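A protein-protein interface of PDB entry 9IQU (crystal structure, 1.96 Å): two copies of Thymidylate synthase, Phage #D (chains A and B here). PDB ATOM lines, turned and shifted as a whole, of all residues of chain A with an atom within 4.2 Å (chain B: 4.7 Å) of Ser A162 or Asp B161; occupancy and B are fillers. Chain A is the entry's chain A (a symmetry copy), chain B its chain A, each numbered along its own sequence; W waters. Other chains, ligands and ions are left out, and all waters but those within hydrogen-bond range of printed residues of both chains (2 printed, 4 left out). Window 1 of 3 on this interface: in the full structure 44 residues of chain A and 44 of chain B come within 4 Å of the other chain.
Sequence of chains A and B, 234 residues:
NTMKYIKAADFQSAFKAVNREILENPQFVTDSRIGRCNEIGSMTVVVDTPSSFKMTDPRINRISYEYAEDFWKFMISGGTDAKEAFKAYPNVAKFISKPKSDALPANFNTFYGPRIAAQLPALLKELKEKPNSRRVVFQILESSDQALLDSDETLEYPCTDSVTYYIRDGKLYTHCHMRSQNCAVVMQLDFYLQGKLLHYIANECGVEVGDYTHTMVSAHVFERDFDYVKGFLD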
ATOM      1  N   VAL A 137      23.084   0.782 -26.609  1.00  0.00           N
ATOM      2  CA  VAL A 137      22.803   2.067 -25.998  1.00  0.00           C
ATOM      3  C   VAL A 137      23.524   3.200 -26.709  1.00  0.00           C
ATOM      4  O   VAL A 137      24.760   3.261 -26.700  1.00  0.00           O
ATOM      5  CB  VAL A 137      23.205   2.089 -24.526  1.00  0.00           C
ATOM      6  CG1 VAL A 137      22.894   3.475 -23.930  1.00  0.00           C
ATOM      7  CG2 VAL A 137      22.490   0.987 -23.759  1.00  0.00           C
ATOM      8  N   PHE A 138      22.756   4.119 -27.282  1.00  0.00           N
ATOM      9  CA  PHE A 138      23.336   5.340 -27.840  1.00  0.00           C
ATOM     10  C   PHE A 138      23.593   6.347 -26.726  1.00  0.00           C
ATOM     11  O   PHE A 138      22.661   6.752 -26.018  1.00  0.00           O
ATOM     12  CB  PHE A 138      22.408   5.958 -28.885  1.00  0.00           C
ATOM     13  CG  PHE A 138      22.422   5.259 -30.226  1.00  0.00           C
ATOM     14  CD1 PHE A 138      21.554   4.219 -30.494  1.00  0.00           C
ATOM     15  CD2 PHE A 138      23.280   5.679 -31.236  1.00  0.00           C
ATOM     16  CE1 PHE A 138      21.564   3.584 -31.729  1.00  0.00           C
ATOM     17  CE2 PHE A 138      23.282   5.048 -32.481  1.00  0.00           C
ATOM     18  CZ  PHE A 138      22.423   4.006 -32.723  1.00  0.00           C
ATOM     19  N   GLN A 139      24.841   6.760 -26.546  1.00  0.00           N
ATOM     20  CA  GLN A 139      25.114   7.827 -25.581  1.00  0.00           C
ATOM     21  C   GLN A 139      24.905   9.144 -26.283  1.00  0.00           C
ATOM     22  O   GLN A 139      25.441   9.359 -27.371  1.00  0.00           O
ATOM     23  CB  GLN A 139      26.540   7.760 -25.034  1.00  0.00           C
ATOM     24  CG  GLN A 139      26.865   6.463 -24.348  1.00  0.00           C
ATOM     25  CD  GLN A 139      26.046   6.253 -23.099  1.00  0.00           C
ATOM     26  OE1 GLN A 139      25.732   7.201 -22.384  1.00  0.00           O
ATOM     27  NE2 GLN A 139      25.669   5.002 -22.843  1.00  0.00           N
ATOM     28  N   THR A 160      19.243  14.966 -23.440  1.00  0.00           N
ATOM     29  CA  THR A 160      19.059  13.538 -23.667  1.00  0.00           C
ATOM     30  C   THR A 160      20.300  12.796 -23.200  1.00  0.00           C
ATOM     31  O   THR A 160      21.399  13.080 -23.660  1.00  0.00           O
ATOM     32  CB  THR A 160      18.792  13.258 -25.173  1.00  0.00           C
ATOM     33  OG1 THR A 160      17.640  13.997 -25.602  1.00  0.00           O
ATOM     34  CG2 THR A 160      18.580  11.760 -25.446  1.00  0.00           C
ATOM     35  N   ASP A 161      20.129  11.860 -22.268  1.00  0.00           N
ATOM     36  CA  ASP A 161      21.261  11.125 -21.703  1.00  0.00           C
ATOM     37  C   ASP A 161      21.633   9.928 -22.584  1.00  0.00           C
ATOM     38  O   ASP A 161      22.777   9.792 -23.018  1.00  0.00           O
ATOM     39  CB  ASP A 161      20.931  10.684 -20.275  1.00  0.00           C
ATOM     40  CG  ASP A 161      22.163  10.336 -19.474  1.00  0.00           C
ATOM     41  OD1 ASP A 161      22.030   9.736 -18.389  1.00  0.00           O
ATOM     42  OD2 ASP A 161      23.271  10.680 -19.917  1.00  0.00           O
ATOM     43  N   SER A 162      20.655   9.087 -22.895  1.00  0.00           N
ATOM     44  CA  SER A 162      20.910   7.944 -23.751  1.00  0.00           C
ATOM     45  C   SER A 162      19.612   7.372 -24.300  1.00  0.00           C
ATOM     46  O   SER A 162      18.533   7.662 -23.778  1.00  0.00           O
ATOM     47  CB  SER A 162      21.662   6.849 -22.994  1.00  0.00           C
ATOM     48  OG  SER A 162      20.833   6.228 -22.026  1.00  0.00           O
ATOM     49  N   VAL A 163      19.740   6.550 -25.340  1.00  0.00           N
ATOM     50  CA  VAL A 163      18.603   5.894 -25.969  1.00  0.00           C
ATOM     51  C   VAL A 163      18.975   4.418 -26.086  1.00  0.00           C
ATOM     52  O   VAL A 163      19.965   4.078 -26.740  1.00  0.00           O
ATOM     53  CB  VAL A 163      18.281   6.493 -27.358  1.00  0.00           C
ATOM     54  CG1 VAL A 163      17.120   5.756 -28.002  1.00  0.00           C
ATOM     55  CG2 VAL A 163      18.028   8.004 -27.268  1.00  0.00           C
ATOM     56  N   HIS A 175      14.017   2.610 -25.112  1.00  0.00           N
ATOM     57  CA  HIS A 175      13.997   3.382 -23.868  1.00  0.00           C
ATOM     58  C   HIS A 175      14.876   4.628 -23.984  1.00  0.00           C
ATOM     59  O   HIS A 175      16.099   4.542 -23.998  1.00  0.00           O
ATOM     60  CB  HIS A 175      14.460   2.539 -22.669  1.00  0.00           C
ATOM     61  CG  HIS A 175      14.287   3.234 -21.353  1.00  0.00           C
ATOM     62  ND1 HIS A 175      13.547   2.696 -20.322  1.00  0.00           N
ATOM     63  CD2 HIS A 175      14.727   4.440 -20.913  1.00  0.00           C
ATOM     64  CE1 HIS A 175      13.563   3.527 -19.292  1.00  0.00           C
ATOM     65  NE2 HIS A 175      14.260   4.600 -19.628  1.00  0.00           N
ATOM     66  N   CYS A 176      14.231   5.788 -24.050  1.00  0.00           N
ATOM     67  CA  CYS A 176      14.919   7.070 -24.058  1.00  0.00           C
ATOM     68  C   CYS A 176      15.019   7.639 -22.643  1.00  0.00           C
ATOM     69  O   CYS A 176      13.991   7.891 -22.004  1.00  0.00           O
ATOM     70  CB  CYS A 176      14.185   8.049 -24.987  1.00  0.00           C
ATOM     71  SG  CYS A 176      14.836   9.751 -24.967  1.00  0.00           S
ATOM     72  N   HIS A 177      16.245   7.825 -22.150  1.00  0.00           N
ATOM     73  CA  HIS A 177      16.457   8.445 -20.831  1.00  0.00           C
ATOM     74  C   HIS A 177      16.876   9.905 -20.953  1.00  0.00           C
ATOM     75  O   HIS A 177      17.935  10.209 -21.506  1.00  0.00           O
ATOM     76  CB  HIS A 177      17.514   7.682 -20.025  1.00  0.00           C
ATOM     77  CG  HIS A 177      17.645   8.161 -18.607  1.00  0.00           C
ATOM     78  ND1 HIS A 177      16.587   8.177 -17.728  1.00  0.00           N
ATOM     79  CD2 HIS A 177      18.713   8.647 -17.920  1.00  0.00           C
ATOM     80  CE1 HIS A 177      16.999   8.627 -16.551  1.00  0.00           C
ATOM     81  NE2 HIS A 177      18.281   8.937 -16.650  1.00  0.00           N
ATOM     82  N   PHE B 138      26.532  11.661 -13.493  1.00  0.00           N
ATOM     83  CA  PHE B 138      27.726  10.827 -13.633  1.00  0.00           C
ATOM     84  C   PHE B 138      27.533   9.835 -14.772  1.00  0.00           C
ATOM     85  O   PHE B 138      26.599   9.023 -14.746  1.00  0.00           O
ATOM     86  CB  PHE B 138      28.018  10.071 -12.337  1.00  0.00           C
ATOM     87  CG  PHE B 138      28.650  10.911 -11.251  1.00  0.00           C
ATOM     88  CD1 PHE B 138      27.873  11.592 -10.336  1.00  0.00           C
ATOM     89  CD2 PHE B 138      30.034  10.981 -11.123  1.00  0.00           C
ATOM     90  CE1 PHE B 138      28.457  12.357  -9.335  1.00  0.00           C
ATOM     91  CE2 PHE B 138      30.621  11.741 -10.109  1.00  0.00           C
ATOM     92  CZ  PHE B 138      29.830  12.422  -9.218  1.00  0.00           C
ATOM     93  N   GLN B 139      28.394   9.883 -15.782  1.00  0.00           N
ATOM     94  CA  GLN B 139      28.331   8.861 -16.829  1.00  0.00           C
ATOM     95  C   GLN B 139      29.130   7.674 -16.360  1.00  0.00           C
ATOM     96  O   GLN B 139      30.275   7.826 -15.933  1.00  0.00           O
ATOM     97  CB  GLN B 139      28.894   9.363 -18.159  1.00  0.00           C
ATOM     98  CG  GLN B 139      28.189  10.577 -18.696  1.00  0.00           C
ATOM     99  CD  GLN B 139      26.753  10.294 -19.058  1.00  0.00           C
ATOM    100  OE1 GLN B 139      26.421   9.205 -19.518  1.00  0.00           O
ATOM    101  NE2 GLN B 139      25.881  11.272 -18.822  1.00  0.00           N
ATOM    102  N   ILE B 140      28.538   6.493 -16.413  1.00  0.00           N
ATOM    103  CA  ILE B 140      29.324   5.285 -16.183  1.00  0.00           C
ATOM    104  C   ILE B 140      29.605   4.664 -17.556  1.00  0.00           C
ATOM    105  O   ILE B 140      30.738   4.727 -18.066  1.00  0.00           O
ATOM    106  CB  ILE B 140      28.604   4.318 -15.257  1.00  0.00           C
ATOM    107  CG1 ILE B 140      28.233   5.023 -13.943  1.00  0.00           C
ATOM    108  CG2 ILE B 140      29.441   3.032 -15.054  1.00  0.00           C
ATOM    109  CD1 ILE B 140      29.402   5.545 -13.137  1.00  0.00           C
ATOM    110  N   LEU B 141      28.565   4.108 -18.173  1.00  0.00           N
ATOM    111  CA  LEU B 141      28.682   3.606 -19.545  1.00  0.00           C
ATOM    112  C   LEU B 141      28.922   4.794 -20.478  1.00  0.00           C
ATOM    113  O   LEU B 141      28.160   5.764 -20.428  1.00  0.00           O
ATOM    114  CB  LEU B 141      27.413   2.836 -19.946  1.00  0.00           C
ATOM    115  CG  LEU B 141      27.311   2.272 -21.369  1.00  0.00           C
ATOM    116  CD1 LEU B 141      28.413   1.252 -21.577  1.00  0.00           C
ATOM    117  CD2 LEU B 141      25.913   1.635 -21.628  1.00  0.00           C
ATOM    118  N   CYS B 159      27.037  -2.065 -16.877  1.00  0.00           N
ATOM    119  CA  CYS B 159      25.620  -2.302 -16.701  1.00  0.00           C
ATOM    120  C   CYS B 159      24.891  -1.035 -16.255  1.00  0.00           C
ATOM    121  O   CYS B 159      23.696  -0.881 -16.493  1.00  0.00           O
ATOM    122  CB  CYS B 159      25.415  -3.426 -15.678  1.00  0.00           C
ATOM    123  SG  CYS B 159      26.252  -4.940 -16.144  1.00  0.00           S
ATOM    124  N   THR B 160      25.631  -0.151 -15.598  1.00  0.00           N
ATOM    125  CA  THR B 160      25.139   1.129 -15.105  1.00  0.00           C
ATOM    126  C   THR B 160      25.386   2.197 -16.159  1.00  0.00           C
ATOM    127  O   THR B 160      26.519   2.400 -16.576  1.00  0.00           O
ATOM    128  CB  THR B 160      25.845   1.506 -13.772  1.00  0.00           C
ATOM    129  OG1 THR B 160      25.631   0.468 -12.806  1.00  0.00           O
ATOM    130  CG2 THR B 160      25.338   2.847 -13.217  1.00  0.00           C
ATOM    131  N   ASP B 161      24.324   2.864 -16.605  1.00  0.00           N
ATOM    132  CA  ASP B 161      24.437   3.870 -17.660  1.00  0.00           C
ATOM    133  C   ASP B 161      24.825   5.234 -17.078  1.00  0.00           C
ATOM    134  O   ASP B 161      25.818   5.837 -17.485  1.00  0.00           O
ATOM    135  CB  ASP B 161      23.124   3.952 -18.441  1.00  0.00           C
ATOM    136  CG  ASP B 161      23.290   4.606 -19.793  1.00  0.00           C
ATOM    137  OD1 ASP B 161      22.273   4.954 -20.425  1.00  0.00           O
ATOM    138  OD2 ASP B 161      24.440   4.756 -20.237  1.00  0.00           O
ATOM    139  N   SER B 162      24.075   5.697 -16.088  1.00  0.00           N
ATOM    140  CA  SER B 162      24.388   6.965 -15.455  1.00  0.00           C
ATOM    141  C   SER B 162      23.679   7.097 -14.116  1.00  0.00           C
ATOM    142  O   SER B 162      22.727   6.364 -13.839  1.00  0.00           O
ATOM    143  CB  SER B 162      23.994   8.136 -16.352  1.00  0.00           C
ATOM    144  OG  SER B 162      22.584   8.269 -16.440  1.00  0.00           O
ATOM    145  N   HIS B 177      20.203   5.149 -13.574  1.00  0.00           N
ATOM    146  CA  HIS B 177      19.707   4.467 -14.781  1.00  0.00           C
ATOM    147  C   HIS B 177      20.595   3.292 -15.173  1.00  0.00           C
ATOM    148  O   HIS B 177      21.769   3.477 -15.499  1.00  0.00           O
ATOM    149  CB  HIS B 177      19.603   5.438 -15.962  1.00  0.00           C
ATOM    150  CG  HIS B 177      18.936   4.842 -17.169  1.00  0.00           C
ATOM    151  ND1 HIS B 177      17.664   4.318 -17.132  1.00  0.00           N
ATOM    152  CD2 HIS B 177      19.370   4.685 -18.448  1.00  0.00           C
ATOM    153  CE1 HIS B 177      17.331   3.885 -18.340  1.00  0.00           C
ATOM    154  NE2 HIS B 177      18.358   4.080 -19.150  1.00  0.00           N
ATOM    155  N   MET B 178      20.015   2.093 -15.100  1.00  0.00           N
ATOM    156  CA  MET B 178      20.686   0.816 -15.371  1.00  0.00           C
ATOM    157  C   MET B 178      20.358   0.403 -16.816  1.00  0.00           C
ATOM    158  O   MET B 178      19.195   0.321 -17.205  1.00  0.00           O
ATOM    159  CB  MET B 178      20.184  -0.266 -14.396  1.00  0.00           C
ATOM    160  CG  MET B 178      20.656  -0.034 -12.941  1.00  0.00           C
ATOM    161  SD  MET B 178      22.414   0.094 -12.640  1.00  0.00           S
ATOM    162  CE  MET B 178      23.054  -1.554 -12.927  1.00  0.00           C
ATOM    163  N   ARG B 179      21.385   0.135 -17.602  1.00  0.00           N
ATOM    164  CA  ARG B 179      21.202  -0.486 -18.894  1.00  0.00           C
ATOM    165  C   ARG B 179      20.697  -1.920 -18.701  1.00  0.00           C
ATOM    166  O   ARG B 179      19.744  -2.367 -19.346  1.00  0.00           O
ATOM    167  CB  ARG B 179      22.526  -0.470 -19.675  1.00  0.00           C
ATOM    168  CG  ARG B 179      22.528  -1.393 -20.900  1.00  0.00           C
ATOM    169  CD  ARG B 179      23.925  -1.538 -21.486  1.00  0.00           C
ATOM    170  NE  ARG B 179      24.813  -2.354 -20.662  1.00  0.00           N
ATOM    171  CZ  ARG B 179      24.767  -3.680 -20.609  1.00  0.00           C
ATOM    172  NH1 ARG B 179      23.883  -4.366 -21.306  1.00  0.00           N
ATOM    173  NH2 ARG B 179      25.645  -4.334 -19.848  1.00  0.00           N
HETATM  174  O   HOH W   1      18.493   4.584 -22.260  1.00  0.00           O
HETATM  175  O   HOH W   2      20.589   8.966 -14.501  1.00  0.00           O
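O of Leu B141 lies close to OE1 of Gln A139, at 3.4 Å.
The side-chain carboxylate of Asp B161 lies within hydrogen-bond range of the side-chain hydroxyl of Ser A162 (2.5 Å).
The side-chain carboxylate of Asp A161 is in hydrogen-bond range of the side-chain amide nitrogen of Gln B139, 2.9 Å away.
OD1 of Asp A161 lies within hydrogen-bond range of OG of Ser B162.
The side-chain carboxylate of Asp B161 sits at hydrogen-bond distance from the side-chain amide nitrogen of Gln A139.
O of Cys B159 sits at hydrogen-bond distance from N of Arg B179 (2.8 Å).
The backbone NH (N) of Asp A161 lies within hydrogen-bond range of the backbone carbonyl oxygen (O) of His A177.
The backbone carbonyl oxygen of Ser B162 sits at hydrogen-bond distance from the backbone NH of His B177.
N of His A177 sits at hydrogen-bond distance from O of Ser A162, at 2.8 Å.
The backbone NH (N) of Leu B141 sits at hydrogen-bond distance from the backbone carbonyl oxygen (O) of Asp B161 (3.3 Å).
The backbone carbonyl oxygen of Thr B160 is in hydrogen-bond range of the backbone NH of Leu B141 (3.1 Å).
Among the printed residues, merely in contact across the chains: His A175 with His B177 (3.4 Å), Gln A139 with Gln B139 (3.6 Å), Val A137 with Arg B179 (3.7 Å), His A177 with His B177 (3.8 Å), Val A137 with Asp B161 (3.9 Å) and Val A137 with Leu B141 (3.99 Å).
Ser A162 touches just one residue of chain B: Asp B161.
Asp B161 touches three residues of chain A.
Printed residues of chain B within 4 Å of Val A137: Leu B141 (3.99 Å), Asp B161 (3.9 Å) and Arg B179 (3.7 Å).
Printed residues of chain B within 4 Å of Gln A139: Gln B139 (3.6 Å), Leu B141 (3.4 Å) and Asp B161 (2.9 Å).
Of the printed residues of chain A, His B177 touches His A175 and His A177.
Of the printed residues of chain B, His A175 touches His B177.
The nearest residue of chain B that does not touch Ser A162 is His B177 (4.2 Å).
Of the 10 printed residues of chain A, 6 touch a printed residue of chain B.
Printed residues of chain A that touch a printed residue of chain B: Val A137, Gln A139, Asp A161, Ser A162, His A175 and His A177.
Along chain A the printed residues that touch a printed residue of chain B span positions 137 to 177.
Printed residues of chain B that touch a printed residue of chain A: Gln B139, Leu B141, Asp B161, Ser B162, His B177 and Arg B179.
Hydrophobic or aromatic side chains of chain B that line the printed part of chain A: Leu B141 and His B177.
Among the printed residues, 11 pairs touch across the chains.
Gln A139 touches its own counterpart, Gln B139.
Gln A139 touches Asp B161, and with the chains exchanged Asp A161 touches Gln B139.
Asp A161 touches Ser B162, and with the chains exchanged Ser A162 touches Asp B161.
His A177 touches its own counterpart, His B177.
Of the 11 pairs that touch across the chains among the printed residues, 6 have their exchanged pair printed and touching as well.
Water W2 lies within hydrogen-bond range of OG of Ser B162 (2.9 Å) and NE2 of His A177 (3.2 Å).
Water W1 lies within hydrogen-bond range of OG of Ser A162, O of His A175 and NE2 of His B177.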
